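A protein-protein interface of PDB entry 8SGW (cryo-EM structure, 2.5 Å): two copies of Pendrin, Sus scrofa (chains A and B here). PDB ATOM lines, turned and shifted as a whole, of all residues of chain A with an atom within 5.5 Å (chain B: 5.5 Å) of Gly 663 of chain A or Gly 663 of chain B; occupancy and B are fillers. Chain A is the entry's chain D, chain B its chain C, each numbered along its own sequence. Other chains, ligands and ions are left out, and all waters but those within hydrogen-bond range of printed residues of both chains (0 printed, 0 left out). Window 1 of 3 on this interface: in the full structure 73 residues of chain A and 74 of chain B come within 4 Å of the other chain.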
ATOM      1  N   ARG A 549       5.799  19.455  31.853  1.00  0.00           N
ATOM      2  CA  ARG A 549       5.820  18.337  30.923  1.00  0.00           C
ATOM      3  C   ARG A 549       5.714  17.045  31.721  1.00  0.00           C
ATOM      4  O   ARG A 549       6.563  16.771  32.577  1.00  0.00           O
ATOM      5  CB  ARG A 549       7.088  18.337  30.073  1.00  0.00           C
ATOM      6  CG  ARG A 549       7.385  16.990  29.440  1.00  0.00           C
ATOM      7  CD  ARG A 549       8.244  17.125  28.200  1.00  0.00           C
ATOM      8  NE  ARG A 549       8.228  15.906  27.400  1.00  0.00           N
ATOM      9  CZ  ARG A 549       7.736  15.822  26.171  1.00  0.00           C
ATOM     10  NH1 ARG A 549       7.206  16.871  25.565  1.00  0.00           N
ATOM     11  NH2 ARG A 549       7.780  14.657  25.533  1.00  0.00           N
ATOM     12  N   ASP A 661       2.457  20.441  29.096  1.00  0.00           N
ATOM     13  CA  ASP A 661       3.127  19.886  27.924  1.00  0.00           C
ATOM     14  C   ASP A 661       2.822  18.395  27.873  1.00  0.00           C
ATOM     15  O   ASP A 661       3.401  17.603  28.619  1.00  0.00           O
ATOM     16  CB  ASP A 661       4.627  20.149  27.985  1.00  0.00           C
ATOM     17  CG  ASP A 661       5.366  19.610  26.774  1.00  0.00           C
ATOM     18  OD1 ASP A 661       4.709  19.280  25.764  1.00  0.00           O
ATOM     19  OD2 ASP A 661       6.610  19.521  26.830  1.00  0.00           O
ATOM     20  N   CYS A 662       1.906  18.010  26.992  1.00  0.00           N
ATOM     21  CA  CYS A 662       1.444  16.633  26.875  1.00  0.00           C
ATOM     22  C   CYS A 662       1.959  15.978  25.597  1.00  0.00           C
ATOM     23  O   CYS A 662       1.256  15.196  24.956  1.00  0.00           O
ATOM     24  CB  CYS A 662      -0.078  16.570  26.933  1.00  0.00           C
ATOM     25  SG  CYS A 662      -0.812  17.496  28.298  1.00  0.00           S
ATOM     26  N   GLY A 663       3.193  16.302  25.214  1.00  0.00           N
ATOM     27  CA  GLY A 663       3.758  15.716  24.011  1.00  0.00           C
ATOM     28  C   GLY A 663       3.944  14.215  24.119  1.00  0.00           C
ATOM     29  O   GLY A 663       3.761  13.485  23.143  1.00  0.00           O
ATOM     30  N   ALA A 664       4.304  13.735  25.306  1.00  0.00           N
ATOM     31  CA  ALA A 664       4.573  12.320  25.516  1.00  0.00           C
ATOM     32  C   ALA A 664       3.375  11.548  26.049  1.00  0.00           C
ATOM     33  O   ALA A 664       3.506  10.352  26.328  1.00  0.00           O
ATOM     34  CB  ALA A 664       5.758  12.145  26.465  1.00  0.00           C
ATOM     35  N   VAL A 665       2.218  12.189  26.201  1.00  0.00           N
ATOM     36  CA  VAL A 665       1.018  11.484  26.645  1.00  0.00           C
ATOM     37  C   VAL A 665       0.561  10.573  25.508  1.00  0.00           C
ATOM     38  O   VAL A 665       0.052  11.045  24.488  1.00  0.00           O
ATOM     39  CB  VAL A 665      -0.088  12.458  27.064  1.00  0.00           C
ATOM     40  CG1 VAL A 665      -1.372  11.704  27.360  1.00  0.00           C
ATOM     41  CG2 VAL A 665       0.349  13.258  28.277  1.00  0.00           C
ATOM     42  N   ALA A 693      -0.959  21.498  25.535  1.00  0.00           N
ATOM     43  CA  ALA A 693      -0.172  21.670  24.324  1.00  0.00           C
ATOM     44  C   ALA A 693       0.466  20.351  23.921  1.00  0.00           C
ATOM     45  O   ALA A 693       0.689  19.468  24.755  1.00  0.00           O
ATOM     46  CB  ALA A 693       0.910  22.739  24.508  1.00  0.00           C
ATOM     47  N   SER A 694       0.747  20.227  22.623  1.00  0.00           N
ATOM     48  CA  SER A 694       1.446  19.087  22.031  1.00  0.00           C
ATOM     49  C   SER A 694       0.660  17.785  22.142  1.00  0.00           C
ATOM     50  O   SER A 694       1.241  16.699  22.054  1.00  0.00           O
ATOM     51  CB  SER A 694       2.842  18.915  22.640  1.00  0.00           C
ATOM     52  OG  SER A 694       3.673  20.019  22.329  1.00  0.00           O
ATOM     53  N   LEU A 695      -0.655  17.862  22.326  1.00  0.00           N
ATOM     54  CA  LEU A 695      -1.468  16.655  22.368  1.00  0.00           C
ATOM     55  C   LEU A 695      -1.625  16.070  20.973  1.00  0.00           C
ATOM     56  O   LEU A 695      -1.785  16.796  19.989  1.00  0.00           O
ATOM     57  CB  LEU A 695      -2.844  16.946  22.960  1.00  0.00           C
ATOM     58  CG  LEU A 695      -2.950  16.995  24.481  1.00  0.00           C
ATOM     59  CD1 LEU A 695      -2.437  18.323  24.988  1.00  0.00           C
ATOM     60  CD2 LEU A 695      -4.384  16.760  24.923  1.00  0.00           C
ATOM     61  N   GLN A 696      -1.585  14.745  20.893  1.00  0.00           N
ATOM     62  CA  GLN A 696      -1.796  14.072  19.625  1.00  0.00           C
ATOM     63  C   GLN A 696      -3.278  14.077  19.259  1.00  0.00           C
ATOM     64  O   GLN A 696      -4.154  14.277  20.105  1.00  0.00           O
ATOM     65  CB  GLN A 696      -1.265  12.642  19.681  1.00  0.00           C
ATOM     66  CG  GLN A 696       0.243  12.543  19.532  1.00  0.00           C
ATOM     67  CD  GLN A 696       0.764  13.368  18.374  1.00  0.00           C
ATOM     68  OE1 GLN A 696       1.412  14.395  18.571  1.00  0.00           O
ATOM     69  NE2 GLN A 696       0.483  12.921  17.155  1.00  0.00           N
ATOM     70  N   ARG B 549       6.152   8.880  13.357  1.00  0.00           N
ATOM     71  CA  ARG B 549       5.930   9.149  14.769  1.00  0.00           C
ATOM     72  C   ARG B 549       5.425   7.874  15.428  1.00  0.00           C
ATOM     73  O   ARG B 549       4.384   7.337  15.030  1.00  0.00           O
ATOM     74  CB  ARG B 549       4.934  10.288  14.974  1.00  0.00           C
ATOM     75  CG  ARG B 549       4.318  10.301  16.361  1.00  0.00           C
ATOM     76  CD  ARG B 549       3.821  11.680  16.744  1.00  0.00           C
ATOM     77  NE  ARG B 549       3.570  11.783  18.177  1.00  0.00           N
ATOM     78  CZ  ARG B 549       4.233  12.587  18.997  1.00  0.00           C
ATOM     79  NH1 ARG B 549       5.200  13.376  18.561  1.00  0.00           N
ATOM     80  NH2 ARG B 549       3.915  12.600  20.289  1.00  0.00           N
ATOM     81  N   ASP B 661      10.104  10.437  14.667  1.00  0.00           N
ATOM     82  CA  ASP B 661       9.526  11.384  15.618  1.00  0.00           C
ATOM     83  C   ASP B 661       9.301  10.648  16.931  1.00  0.00           C
ATOM     84  O   ASP B 661       8.350   9.877  17.073  1.00  0.00           O
ATOM     85  CB  ASP B 661       8.229  11.970  15.075  1.00  0.00           C
ATOM     86  CG  ASP B 661       7.601  12.979  16.019  1.00  0.00           C
ATOM     87  OD1 ASP B 661       8.288  13.434  16.958  1.00  0.00           O
ATOM     88  OD2 ASP B 661       6.418  13.322  15.819  1.00  0.00           O
ATOM     89  N   CYS B 662      10.182  10.885  17.898  1.00  0.00           N
ATOM     90  CA  CYS B 662      10.151  10.200  19.185  1.00  0.00           C
ATOM     91  C   CYS B 662       9.704  11.134  20.303  1.00  0.00           C
ATOM     92  O   CYS B 662      10.204  11.069  21.428  1.00  0.00           O
ATOM     93  CB  CYS B 662      11.516   9.599  19.505  1.00  0.00           C
ATOM     94  SG  CYS B 662      12.242   8.639  18.160  1.00  0.00           S
ATOM     95  N   GLY B 663       8.757  12.022  20.000  1.00  0.00           N
ATOM     96  CA  GLY B 663       8.271  12.943  21.013  1.00  0.00           C
ATOM     97  C   GLY B 663       7.563  12.241  22.154  1.00  0.00           C
ATOM     98  O   GLY B 663       7.668  12.653  23.310  1.00  0.00           O
ATOM     99  N   ALA B 664       6.833  11.172  21.847  1.00  0.00           N
ATOM    100  CA  ALA B 664       6.058  10.453  22.847  1.00  0.00           C
ATOM    101  C   ALA B 664       6.787   9.253  23.433  1.00  0.00           C
ATOM    102  O   ALA B 664       6.199   8.530  24.242  1.00  0.00           O
ATOM    103  CB  ALA B 664       4.723  10.003  22.254  1.00  0.00           C
ATOM    104  N   VAL B 665       8.040   9.018  23.051  1.00  0.00           N
ATOM    105  CA  VAL B 665       8.811   7.921  23.630  1.00  0.00           C
ATOM    106  C   VAL B 665       9.139   8.288  25.073  1.00  0.00           C
ATOM    107  O   VAL B 665       9.968   9.165  25.329  1.00  0.00           O
ATOM    108  CB  VAL B 665      10.080   7.634  22.821  1.00  0.00           C
ATOM    109  CG1 VAL B 665      10.941   6.607  23.536  1.00  0.00           C
ATOM    110  CG2 VAL B 665       9.718   7.146  21.430  1.00  0.00           C
ATOM    111  N   ALA B 693      14.299  12.670  16.368  1.00  0.00           N
ATOM    112  CA  ALA B 693      13.872  14.017  16.717  1.00  0.00           C
ATOM    113  C   ALA B 693      12.910  13.973  17.893  1.00  0.00           C
ATOM    114  O   ALA B 693      12.237  12.967  18.131  1.00  0.00           O
ATOM    115  CB  ALA B 693      13.211  14.720  15.527  1.00  0.00           C
ATOM    116  N   SER B 694      12.864  15.083  18.632  1.00  0.00           N
ATOM    117  CA  SER B 694      11.945  15.296  19.749  1.00  0.00           C
ATOM    118  C   SER B 694      12.195  14.346  20.915  1.00  0.00           C
ATOM    119  O   SER B 694      11.304  14.130  21.742  1.00  0.00           O
ATOM    120  CB  SER B 694      10.484  15.199  19.293  1.00  0.00           C
ATOM    121  OG  SER B 694      10.163  16.240  18.387  1.00  0.00           O
ATOM    122  N   LEU B 695      13.392  13.776  21.010  1.00  0.00           N
ATOM    123  CA  LEU B 695      13.714  12.917  22.141  1.00  0.00           C
ATOM    124  C   LEU B 695      13.929  13.746  23.397  1.00  0.00           C
ATOM    125  O   LEU B 695      14.519  14.829  23.355  1.00  0.00           O
ATOM    126  CB  LEU B 695      14.963  12.086  21.855  1.00  0.00           C
ATOM    127  CG  LEU B 695      14.778  10.819  21.024  1.00  0.00           C
ATOM    128  CD1 LEU B 695      14.666  11.177  19.561  1.00  0.00           C
ATOM    129  CD2 LEU B 695      15.926   9.855  21.263  1.00  0.00           C
ATOM    130  N   GLN B 696      13.451  13.229  24.522  1.00  0.00           N
ATOM    131  CA  GLN B 696      13.661  13.896  25.794  1.00  0.00           C
ATOM    132  C   GLN B 696      15.094  13.688  26.274  1.00  0.00           C
ATOM    133  O   GLN B 696      15.802  12.780  25.831  1.00  0.00           O
ATOM    134  CB  GLN B 696      12.668  13.387  26.837  1.00  0.00           C
ATOM    135  CG  GLN B 696      11.279  13.985  26.703  1.00  0.00           C
ATOM    136  CD  GLN B 696      11.312  15.491  26.539  1.00  0.00           C
ATOM    137  OE1 GLN B 696      11.033  16.015  25.461  1.00  0.00           O
ATOM    138  NE2 GLN B 696      11.655  16.195  27.611  1.00  0.00           N
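Of the 10 printed residues of chain B, 4 touch a printed residue of chain A.
Hydrophobic or aromatic side chains of chain B that line the printed part of chain A: Ala 664.
Along chain B the printed residues that touch a printed residue of chain A span positions 549 to 696.
Of the 10 printed residues of chain A, 4 touch a printed residue of chain B.
Hydrophobic or aromatic side chains of chain A that line the printed part of chain B: Ala 664.
Among the printed residues, no Asp or Glu carboxylate lies within 4 Å of a Lys or Arg side-chain nitrogen of the other chain.
Arg 549 of chain A touches Gly 663 of chain B, and with the chains exchanged Gly 663 of chain A touches Arg 549 of chain B.
Gly 663 of chain B touches its own counterpart, Gly 663 of chain A.
Gly 663 of chain A touches Ala 664 of chain B, and with the chains exchanged Ala 664 of chain A touches Gly 663 of chain B.
Ala 664 of chain B touches its own counterpart, Ala 664 of chain A.
Positions printed for both chains: 549, 661, 662, 663, 664, 665, 693, 694, 695 and 696.
Of the 8 pairs that touch across the chains among the printed residues, 8 have their exchanged pair printed and touching as well.
O of Gly 663 of chain A is in hydrogen-bond range of NH2 of Arg 549 of chain B (3.0 Å).
The guanidinium group (NH2) of Arg 549 of chain A is in hydrogen-bond range of the backbone carbonyl oxygen (O) of Gly 663 of chain B (3.0 Å).
The side-chain amide oxygen (OE1) of Gln 696 of chain B lies close to the guanidinium group (NE) of Arg 549 of chain A (3.4 Å).
The guanidinium group (NE) of Arg 549 of chain B sits close to the side-chain amide oxygen (OE1) of Gln 696 of chain A (3.4 Å).
Among the printed residues, pairs that only touch across the chains: Ala 664 of chain A with Ala 664 of chain B (3.6 Å), Gly 663 of chain A with Ala 664 of chain B (3.7 Å), Ala 664 of chain A with Gly 663 of chain B (3.7 Å) and Gly 663 of chain A with Gly 663 of chain B (3.998 Å).
The guanidinium group (NH1) of Arg 549 of chain A is in salt-bridge range of the side-chain carboxylate (OD2) of Asp 661 of chain A (3.0 Å).
The side-chain carboxylate (OD2) of Asp 661 of chain B is in salt-bridge range of the guanidinium group (NH1) of Arg 549 of chain B (3.0 Å).
The backbone NH (N) of Gly 663 of chain A is in hydrogen-bond range of the side-chain carboxylate (OD1) of Asp 661 of chain A (3.4 Å).
N of Gly 663 of chain B lies within hydrogen-bond range of OD1 of Asp 661 of chain B (3.4 Å).
Of the printed residues of chain B, Gln 696 of chain A touches Arg 549.
Of the printed residues of chain A, Ala 664 of chain B touches Gly 663 and Ala 664.
Of the printed residues of chain A, Gln 696 of chain B touches Arg 549 (3.2 Å).
Ser 694 of chain B touches none of the printed residues of chain A.
Asp 661 of chain A touches none of the printed residues of chain B.
The nearest printed residue of chain B that does not touch Gly 663 of chain A is Val 665 of chain B (6.2 Å).
The nearest printed residue of chain B that does not touch Gln 696 of chain A is Asp 661 of chain B (5.8 Å).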
